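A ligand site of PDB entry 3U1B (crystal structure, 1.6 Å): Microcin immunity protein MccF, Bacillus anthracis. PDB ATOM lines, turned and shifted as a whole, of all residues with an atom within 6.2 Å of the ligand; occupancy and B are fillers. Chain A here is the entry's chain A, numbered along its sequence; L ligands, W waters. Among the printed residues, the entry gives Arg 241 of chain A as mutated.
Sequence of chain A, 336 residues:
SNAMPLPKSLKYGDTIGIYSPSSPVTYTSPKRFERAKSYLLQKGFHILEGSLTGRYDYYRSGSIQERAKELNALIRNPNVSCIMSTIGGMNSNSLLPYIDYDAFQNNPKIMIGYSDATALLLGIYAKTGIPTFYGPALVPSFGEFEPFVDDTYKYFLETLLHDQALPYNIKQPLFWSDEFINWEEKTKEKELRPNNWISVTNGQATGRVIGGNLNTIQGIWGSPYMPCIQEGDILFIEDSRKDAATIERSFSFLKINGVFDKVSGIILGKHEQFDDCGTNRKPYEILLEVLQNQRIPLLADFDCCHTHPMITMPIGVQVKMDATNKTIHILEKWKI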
ATOM      1  N   SER A  23       1.892  22.242  15.582  1.00  0.00           N
ATOM      2  CA  SER A  23       0.451  22.534  15.457  1.00  0.00           C
ATOM      3  C   SER A  23       0.257  23.941  14.922  1.00  0.00           C
ATOM      4  O   SER A  23       0.978  24.829  15.365  1.00  0.00           O
ATOM      5  CB  SER A  23      -0.280  22.450  16.795  1.00  0.00           C
ATOM      6  OG  SER A  23      -0.224  21.118  17.364  1.00  0.00           O
ATOM      7  N   SER A  29      -6.121  29.396  16.849  1.00  0.00           N
ATOM      8  CA  SER A  29      -6.404  30.155  18.074  1.00  0.00           C
ATOM      9  C   SER A  29      -5.938  31.585  17.894  1.00  0.00           C
ATOM     10  O   SER A  29      -5.070  32.066  18.632  1.00  0.00           O
ATOM     11  CB  SER A  29      -5.691  29.517  19.265  1.00  0.00           C
ATOM     12  OG  SER A  29      -6.096  28.167  19.440  1.00  0.00           O
ATOM     13  N   ARG A  32      -5.898  34.180  21.080  1.00  0.00           N
ATOM     14  CA  ARG A  32      -4.830  33.994  22.066  1.00  0.00           C
ATOM     15  C   ARG A  32      -3.505  34.386  21.416  1.00  0.00           C
ATOM     16  O   ARG A  32      -2.659  35.041  22.052  1.00  0.00           O
ATOM     17  CB  ARG A  32      -4.798  32.570  22.628  1.00  0.00           C
ATOM     18  CG  ARG A  32      -3.919  32.492  23.842  1.00  0.00           C
ATOM     19  CD  ARG A  32      -3.992  31.129  24.491  1.00  0.00           C
ATOM     20  NE  ARG A  32      -3.201  30.973  25.698  1.00  0.00           N
ATOM     21  CZ  ARG A  32      -3.708  30.741  26.920  1.00  0.00           C
ATOM     22  NH1 ARG A  32      -2.885  30.446  27.934  1.00  0.00           N
ATOM     23  NH2 ARG A  32      -5.029  30.812  27.137  1.00  0.00           N
ATOM     24  N   ILE A  87       3.779  27.135  19.655  1.00  0.00           N
ATOM     25  CA  ILE A  87       3.155  26.060  20.462  1.00  0.00           C
ATOM     26  C   ILE A  87       3.827  24.783  19.998  1.00  0.00           C
ATOM     27  O   ILE A  87       4.528  24.789  18.979  1.00  0.00           O
ATOM     28  CB  ILE A  87       1.628  25.963  20.191  1.00  0.00           C
ATOM     29  CG1 ILE A  87       0.912  25.207  21.300  1.00  0.00           C
ATOM     30  CG2 ILE A  87       1.360  25.317  18.793  1.00  0.00           C
ATOM     31  CD1 ILE A  87      -0.601  25.547  21.387  1.00  0.00           C
ATOM     32  N   GLY A  88       3.544  23.680  20.700  1.00  0.00           N
ATOM     33  CA  GLY A  88       4.029  22.349  20.406  1.00  0.00           C
ATOM     34  C   GLY A  88       3.058  21.583  19.531  1.00  0.00           C
ATOM     35  O   GLY A  88       2.623  22.087  18.470  1.00  0.00           O
ATOM     36  N   GLY A  89       2.836  20.323  19.863  1.00  0.00           N
ATOM     37  CA  GLY A  89       2.227  19.418  18.936  1.00  0.00           C
ATOM     38  C   GLY A  89       2.921  18.086  19.017  1.00  0.00           C
ATOM     39  O   GLY A  89       3.180  17.583  20.101  1.00  0.00           O
ATOM     40  N   TYR A 114       8.684  24.827  24.693  1.00  0.00           N
ATOM     41  CA  TYR A 114       8.518  23.637  25.512  1.00  0.00           C
ATOM     42  C   TYR A 114       7.773  22.535  24.775  1.00  0.00           C
ATOM     43  O   TYR A 114       7.596  22.597  23.555  1.00  0.00           O
ATOM     44  CB  TYR A 114       7.911  23.977  26.893  1.00  0.00           C
ATOM     45  CG  TYR A 114       6.453  24.412  26.967  1.00  0.00           C
ATOM     46  CD1 TYR A 114       5.491  23.568  27.498  1.00  0.00           C
ATOM     47  CD2 TYR A 114       6.062  25.689  26.602  1.00  0.00           C
ATOM     48  CE1 TYR A 114       4.170  23.950  27.602  1.00  0.00           C
ATOM     49  CE2 TYR A 114       4.718  26.096  26.703  1.00  0.00           C
ATOM     50  CZ  TYR A 114       3.794  25.227  27.212  1.00  0.00           C
ATOM     51  OH  TYR A 114       2.499  25.633  27.350  1.00  0.00           O
ATOM     52  N   SER A 115       7.397  21.516  25.519  1.00  0.00           N
ATOM     53  CA  SER A 115       6.632  20.373  24.986  1.00  0.00           C
ATOM     54  C   SER A 115       7.323  19.804  23.738  1.00  0.00           C
ATOM     55  O   SER A 115       8.511  19.431  23.811  1.00  0.00           O
ATOM     56  CB  SER A 115       5.151  20.746  24.771  1.00  0.00           C
ATOM     57  OG  SER A 115       4.960  21.603  23.660  1.00  0.00           O
ATOM     58  N   ASP A 116       6.593  19.657  22.626  1.00  0.00           N
ATOM     59  CA  ASP A 116       7.171  19.043  21.422  1.00  0.00           C
ATOM     60  C   ASP A 116       8.448  19.765  20.925  1.00  0.00           C
ATOM     61  O   ASP A 116       9.318  19.164  20.281  1.00  0.00           O
ATOM     62  CB  ASP A 116       6.108  19.024  20.322  1.00  0.00           C
ATOM     63  CG  ASP A 116       6.590  18.361  19.030  1.00  0.00           C
ATOM     64  OD1 ASP A 116       6.891  17.145  19.037  1.00  0.00           O
ATOM     65  OD2 ASP A 116       6.657  19.078  18.002  1.00  0.00           O
ATOM     66  N   ALA A 137       6.357  29.154  25.383  1.00  0.00           N
ATOM     67  CA  ALA A 137       5.993  29.217  23.969  1.00  0.00           C
ATOM     68  C   ALA A 137       4.972  30.345  23.811  1.00  0.00           C
ATOM     69  O   ALA A 137       4.182  30.599  24.731  1.00  0.00           O
ATOM     70  CB  ALA A 137       5.362  27.855  23.522  1.00  0.00           C
ATOM     71  N   PRO A 140       0.463  29.517  24.253  1.00  0.00           N
ATOM     72  CA  PRO A 140       0.035  29.105  25.612  1.00  0.00           C
ATOM     73  C   PRO A 140       0.598  29.994  26.730  1.00  0.00           C
ATOM     74  O   PRO A 140      -0.123  30.305  27.674  1.00  0.00           O
ATOM     75  CB  PRO A 140       0.559  27.649  25.751  1.00  0.00           C
ATOM     76  CG  PRO A 140       1.657  27.513  24.720  1.00  0.00           C
ATOM     77  CD  PRO A 140       1.326  28.531  23.585  1.00  0.00           C
ATOM     78  N   GLU A 179      -6.126  24.545  35.197  1.00  0.00           N
ATOM     79  CA  GLU A 179      -7.523  24.538  34.701  1.00  0.00           C
ATOM     80  C   GLU A 179      -7.611  24.668  33.175  1.00  0.00           C
ATOM     81  O   GLU A 179      -6.953  25.530  32.579  1.00  0.00           O
ATOM     82  CB  GLU A 179      -8.342  25.650  35.371  1.00  0.00           C
ATOM     83  CG  GLU A 179      -8.628  25.405  36.840  1.00  0.00           C
ATOM     84  CD  GLU A 179      -9.551  26.478  37.456  1.00  0.00           C
ATOM     85  OE1 GLU A 179      -9.313  26.873  38.613  1.00  0.00           O
ATOM     86  OE2 GLU A 179     -10.515  26.915  36.784  1.00  0.00           O
ATOM     87  N   PHE A 180      -8.476  23.862  32.549  1.00  0.00           N
ATOM     88  CA  PHE A 180      -8.526  23.876  31.100  1.00  0.00           C
ATOM     89  C   PHE A 180      -9.695  24.794  30.823  1.00  0.00           C
ATOM     90  O   PHE A 180     -10.821  24.351  30.531  1.00  0.00           O
ATOM     91  CB  PHE A 180      -8.842  22.414  30.679  1.00  0.00           C
ATOM     92  CG  PHE A 180      -8.623  22.104  29.219  1.00  0.00           C
ATOM     93  CD1 PHE A 180      -7.351  21.884  28.728  1.00  0.00           C
ATOM     94  CD2 PHE A 180      -9.694  22.015  28.339  1.00  0.00           C
ATOM     95  CE1 PHE A 180      -7.123  21.599  27.393  1.00  0.00           C
ATOM     96  CE2 PHE A 180      -9.486  21.741  26.999  1.00  0.00           C
ATOM     97  CZ  PHE A 180      -8.203  21.528  26.526  1.00  0.00           C
ATOM     98  N   ILE A 181      -9.365  26.060  30.657  1.00  0.00           N
ATOM     99  CA  ILE A 181     -10.378  27.111  30.483  1.00  0.00           C
ATOM    100  C   ILE A 181      -9.668  28.365  30.076  1.00  0.00           C
ATOM    101  O   ILE A 181      -8.444  28.424  30.208  1.00  0.00           O
ATOM    102  CB  ILE A 181     -11.152  27.354  31.806  1.00  0.00           C
ATOM    103  CG1 ILE A 181     -12.434  28.158  31.590  1.00  0.00           C
ATOM    104  CG2 ILE A 181     -10.289  28.091  32.859  1.00  0.00           C
ATOM    105  CD1 ILE A 181     -13.324  27.603  30.479  1.00  0.00           C
ATOM    106  N   ASN A 182     -10.436  29.410  29.723  1.00  0.00           N
ATOM    107  CA  ASN A 182      -9.890  30.693  29.325  1.00  0.00           C
ATOM    108  C   ASN A 182      -8.836  30.575  28.235  1.00  0.00           C
ATOM    109  O   ASN A 182      -7.778  31.201  28.304  1.00  0.00           O
ATOM    110  CB  ASN A 182      -9.316  31.413  30.538  1.00  0.00           C
ATOM    111  CG  ASN A 182     -10.367  31.665  31.600  1.00  0.00           C
ATOM    112  OD1 ASN A 182     -11.562  31.593  31.323  1.00  0.00           O
ATOM    113  ND2 ASN A 182      -9.927  31.998  32.818  1.00  0.00           N
ATOM    114  N   TRP A 183      -9.119  29.769  27.213  1.00  0.00           N
ATOM    115  CA  TRP A 183      -8.144  29.631  26.147  1.00  0.00           C
ATOM    116  C   TRP A 183      -8.208  30.830  25.177  1.00  0.00           C
ATOM    117  O   TRP A 183      -7.292  31.653  25.140  1.00  0.00           O
ATOM    118  CB  TRP A 183      -8.365  28.304  25.419  1.00  0.00           C
ATOM    119  CG  TRP A 183      -7.358  28.064  24.350  1.00  0.00           C
ATOM    120  CD1 TRP A 183      -7.598  27.995  23.008  1.00  0.00           C
ATOM    121  CD2 TRP A 183      -5.944  27.899  24.519  1.00  0.00           C
ATOM    122  NE1 TRP A 183      -6.414  27.775  22.325  1.00  0.00           N
ATOM    123  CE2 TRP A 183      -5.387  27.720  23.234  1.00  0.00           C
ATOM    124  CE3 TRP A 183      -5.087  27.869  25.648  1.00  0.00           C
ATOM    125  CZ2 TRP A 183      -4.021  27.506  23.018  1.00  0.00           C
ATOM    126  CZ3 TRP A 183      -3.718  27.641  25.431  1.00  0.00           C
ATOM    127  CH2 TRP A 183      -3.203  27.483  24.128  1.00  0.00           C
ATOM    128  N   ASN A 213      10.346  17.582  27.751  1.00  0.00           N
ATOM    129  CA  ASN A 213       9.136  16.803  27.702  1.00  0.00           C
ATOM    130  C   ASN A 213       9.454  15.325  27.411  1.00  0.00           C
ATOM    131  O   ASN A 213      10.003  14.995  26.353  1.00  0.00           O
ATOM    132  CB  ASN A 213       8.287  17.376  26.561  1.00  0.00           C
ATOM    133  CG  ASN A 213       6.921  16.746  26.502  1.00  0.00           C
ATOM    134  OD1 ASN A 213       6.687  15.784  25.741  1.00  0.00           O
ATOM    135  ND2 ASN A 213       5.994  17.273  27.297  1.00  0.00           N
ATOM    136  N   SER A 240       2.312  16.088  30.077  1.00  0.00           N
ATOM    137  CA  SER A 240       1.029  16.753  30.274  1.00  0.00           C
ATOM    138  C   SER A 240      -0.078  15.983  29.556  1.00  0.00           C
ATOM    139  O   SER A 240       0.131  15.395  28.486  1.00  0.00           O
ATOM    140  CB  SER A 240       1.098  18.160  29.681  1.00  0.00           C
ATOM    141  OG  SER A 240       1.370  18.087  28.298  1.00  0.00           O
ATOM    142  N   ARG A 241      -1.263  15.974  30.189  1.00  0.00           N
ATOM    143  CA  ARG A 241      -2.484  15.386  29.627  1.00  0.00           C
ATOM    144  C   ARG A 241      -2.333  13.915  29.189  1.00  0.00           C
ATOM    145  O   ARG A 241      -2.911  13.498  28.198  1.00  0.00           O
ATOM    146  CB  ARG A 241      -2.999  16.276  28.480  1.00  0.00           C
ATOM    147  CG  ARG A 241      -3.357  17.701  28.980  1.00  0.00           C
ATOM    148  CD  ARG A 241      -3.854  18.639  27.829  1.00  0.00           C
ATOM    149  NE  ARG A 241      -5.102  18.126  27.268  1.00  0.00           N
ATOM    150  CZ  ARG A 241      -5.570  18.420  26.063  1.00  0.00           C
ATOM    151  NH1 ARG A 241      -4.895  19.243  25.262  1.00  0.00           N
ATOM    152  NH2 ARG A 241      -6.715  17.891  25.658  1.00  0.00           N
ATOM    153  N   GLU A 272       0.005  18.478  33.959  1.00  0.00           N
ATOM    154  CA  GLU A 272      -1.270  19.117  33.672  1.00  0.00           C
ATOM    155  C   GLU A 272      -2.383  18.076  33.416  1.00  0.00           C
ATOM    156  O   GLU A 272      -2.262  17.229  32.540  1.00  0.00           O
ATOM    157  CB  GLU A 272      -1.108  20.026  32.413  1.00  0.00           C
ATOM    158  CG  GLU A 272      -2.453  20.633  31.937  1.00  0.00           C
ATOM    159  CD  GLU A 272      -2.325  21.291  30.574  1.00  0.00           C
ATOM    160  OE1 GLU A 272      -1.500  20.844  29.761  1.00  0.00           O
ATOM    161  OE2 GLU A 272      -3.039  22.285  30.339  1.00  0.00           O
ATOM    162  N   HIS A 306       3.604  22.249  31.693  1.00  0.00           N
ATOM    163  CA  HIS A 306       2.423  22.809  31.060  1.00  0.00           C
ATOM    164  C   HIS A 306       1.482  23.574  31.994  1.00  0.00           C
ATOM    165  O   HIS A 306       0.535  24.218  31.534  1.00  0.00           O
ATOM    166  CB  HIS A 306       1.632  21.683  30.378  1.00  0.00           C
ATOM    167  CG  HIS A 306       2.265  21.159  29.129  1.00  0.00           C
ATOM    168  ND1 HIS A 306       3.470  20.472  29.112  1.00  0.00           N
ATOM    169  CD2 HIS A 306       1.822  21.183  27.853  1.00  0.00           C
ATOM    170  CE1 HIS A 306       3.732  20.097  27.867  1.00  0.00           C
ATOM    171  NE2 HIS A 306       2.747  20.520  27.085  1.00  0.00           N
ATOM    172  N   HIS A 308       0.447  26.645  34.731  1.00  0.00           N
ATOM    173  CA  HIS A 308       0.728  28.100  34.870  1.00  0.00           C
ATOM    174  C   HIS A 308       0.994  28.507  36.312  1.00  0.00           C
ATOM    175  O   HIS A 308       0.262  28.043  37.186  1.00  0.00           O
ATOM    176  CB  HIS A 308      -0.445  28.922  34.318  1.00  0.00           C
ATOM    177  CG  HIS A 308      -0.592  28.779  32.841  1.00  0.00           C
ATOM    178  ND1 HIS A 308       0.098  29.593  31.951  1.00  0.00           N
ATOM    179  CD2 HIS A 308      -1.299  27.898  32.090  1.00  0.00           C
ATOM    180  CE1 HIS A 308      -0.208  29.227  30.722  1.00  0.00           C
ATOM    181  NE2 HIS A 308      -1.041  28.194  30.778  1.00  0.00           N
HETATM  182  P1  LIG L   1       1.468  21.480  23.558  1.00  0.00           P
HETATM  183  O1  LIG L   1       0.584  20.924  22.466  1.00  0.00           O
HETATM  184  O2  LIG L   1       2.524  22.502  23.193  1.00  0.00           O
HETATM  185  O3  LIG L   1       2.060  20.345  24.368  1.00  0.00           O
HETATM  186  O4  LIG L   1       0.568  22.063  24.702  1.00  0.00           O
HETATM  187  C1  LIG L   1      -0.368  23.055  24.430  1.00  0.00           C
HETATM  188  C2  LIG L   1      -1.061  23.462  25.682  1.00  0.00           C
HETATM  189  O5  LIG L   1      -1.984  24.511  25.377  1.00  0.00           O
HETATM  190  C3  LIG L   1      -1.939  22.394  26.305  1.00  0.00           C
HETATM  191  O6  LIG L   1      -1.212  21.442  27.061  1.00  0.00           O
HETATM  192  C4  LIG L   1      -2.886  23.220  27.139  1.00  0.00           C
HETATM  193  O7  LIG L   1      -2.222  23.681  28.304  1.00  0.00           O
HETATM  194  C5  LIG L   1      -3.111  24.414  26.208  1.00  0.00           C
HETATM  195  N1  LIG L   1      -4.301  24.268  25.341  1.00  0.00           N
HETATM  196  C6  LIG L   1      -4.314  23.976  24.036  1.00  0.00           C
HETATM  197  N2  LIG L   1      -5.591  24.020  23.579  1.00  0.00           N
HETATM  198  C7  LIG L   1      -6.371  24.389  24.606  1.00  0.00           C
HETATM  199  C8  LIG L   1      -7.807  24.609  24.822  1.00  0.00           C
HETATM  200  N3  LIG L   1      -8.669  24.445  23.791  1.00  0.00           N
HETATM  201  N4  LIG L   1      -8.207  24.960  26.066  1.00  0.00           N
HETATM  202  C9  LIG L   1      -7.349  25.124  27.087  1.00  0.00           C
HETATM  203  N5  LIG L   1      -6.019  24.930  26.947  1.00  0.00           N
HETATM  204  C10 LIG L   1      -5.523  24.543  25.765  1.00  0.00           C
HETATM  205  O   HOH W   1      -1.948  26.797  28.510  1.00  0.00           O
HETATM  206  O   HOH W   2       3.833  24.742  23.823  1.00  0.00           O
HETATM  207  O   HOH W   3      -0.443  18.792  26.137  1.00  0.00           O
HETATM  208  O   HOH W   4       3.570  18.856  22.490  1.00  0.00           O
HETATM  209  O   HOH W   5       0.426  17.991  22.221  1.00  0.00           O
HETATM  210  O   HOH W   6     -10.816  25.543  26.873  1.00  0.00           O
HETATM  211  O   HOH W   7      -4.797  26.091  29.277  1.00  0.00           O
HETATM  212  O   HOH W   8      -0.456  21.569  20.120  1.00  0.00           O
HETATM  213  O   HOH W   9       0.439  24.684  28.778  1.00  0.00           O
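N of Gly 88 is in hydrogen-bond range of O2 of the ligand (2.9 Å).
The side-chain carboxylate of Glu 272 sits at hydrogen-bond distance from an oxygen (O7) of the ligand, at 2.6 Å.
NE2 of His 306 is in hydrogen-bond range of O3 of the ligand (2.8 Å).
The backbone NH (N) of Gly 89 sits at hydrogen-bond distance from an oxygen (O1) of the ligand, 3.5 Å away.
An oxygen (O2) of the ligand lies within hydrogen-bond range of the side-chain hydroxyl (OG) of Ser 115 (2.6 Å).
O of Trp 183 is in hydrogen-bond range of NH2 of Arg 32, 3.1 Å away.
The indole nitrogen (NE1) of Trp 183 lies within hydrogen-bond range of the side-chain hydroxyl (OG) of Ser 29 (2.9 Å).
N of Ser 23 sits at hydrogen-bond distance from O of Gly 88 (3.0 Å).
NE2 of His 306 lies within hydrogen-bond range of OG of Ser 240 (3.0 Å).
The backbone carbonyl oxygen (O) of Glu 272 sits at hydrogen-bond distance from the backbone NH (N) of Arg 241 (2.8 Å).
Ile 87 touches the ligand.
CZ of Phe 180 touches N4 of the ligand, 3.5 Å away.
Trp 183 touches the ligand.
Arg 241 touches the ligand.
Hydrophobic or aromatic side chains that line the ligand: Ile 87, Phe 180, Trp 183 and His 306.
Within 4 Å of the ligand: Ile 87, Gly 88, Gly 89, Ser 115, Phe 180, Trp 183, Arg 241, Glu 272 and His 306.
The nearest printed residue that does not touch the ligand is Pro 140 (4.1 Å).
Water W8 lies within hydrogen-bond range of O1 of the ligand and OG of Ser 23.
Water W2 lies within hydrogen-bond range of O2 of the ligand, N of Gly 88 and OG of Ser 115.
Water W4 lies within hydrogen-bond range of the backbone carbonyl oxygen (O) of Gly 89, an oxygen (O3) of the ligand, the backbone NH (N) of Asp 116 and the side-chain hydroxyl (OG) of Ser 115.
Water W3 lies within hydrogen-bond range of OG of Ser 240 (2.9 Å) and O6 of the ligand (2.9 Å).
Water W5 lies within hydrogen-bond range of an oxygen (O1) of the ligand (2.9 Å) and the backbone carbonyl oxygen of Gly 89 (3.5 Å).
Water W1 bridges NE2 of His 308 and O7 of the ligand.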
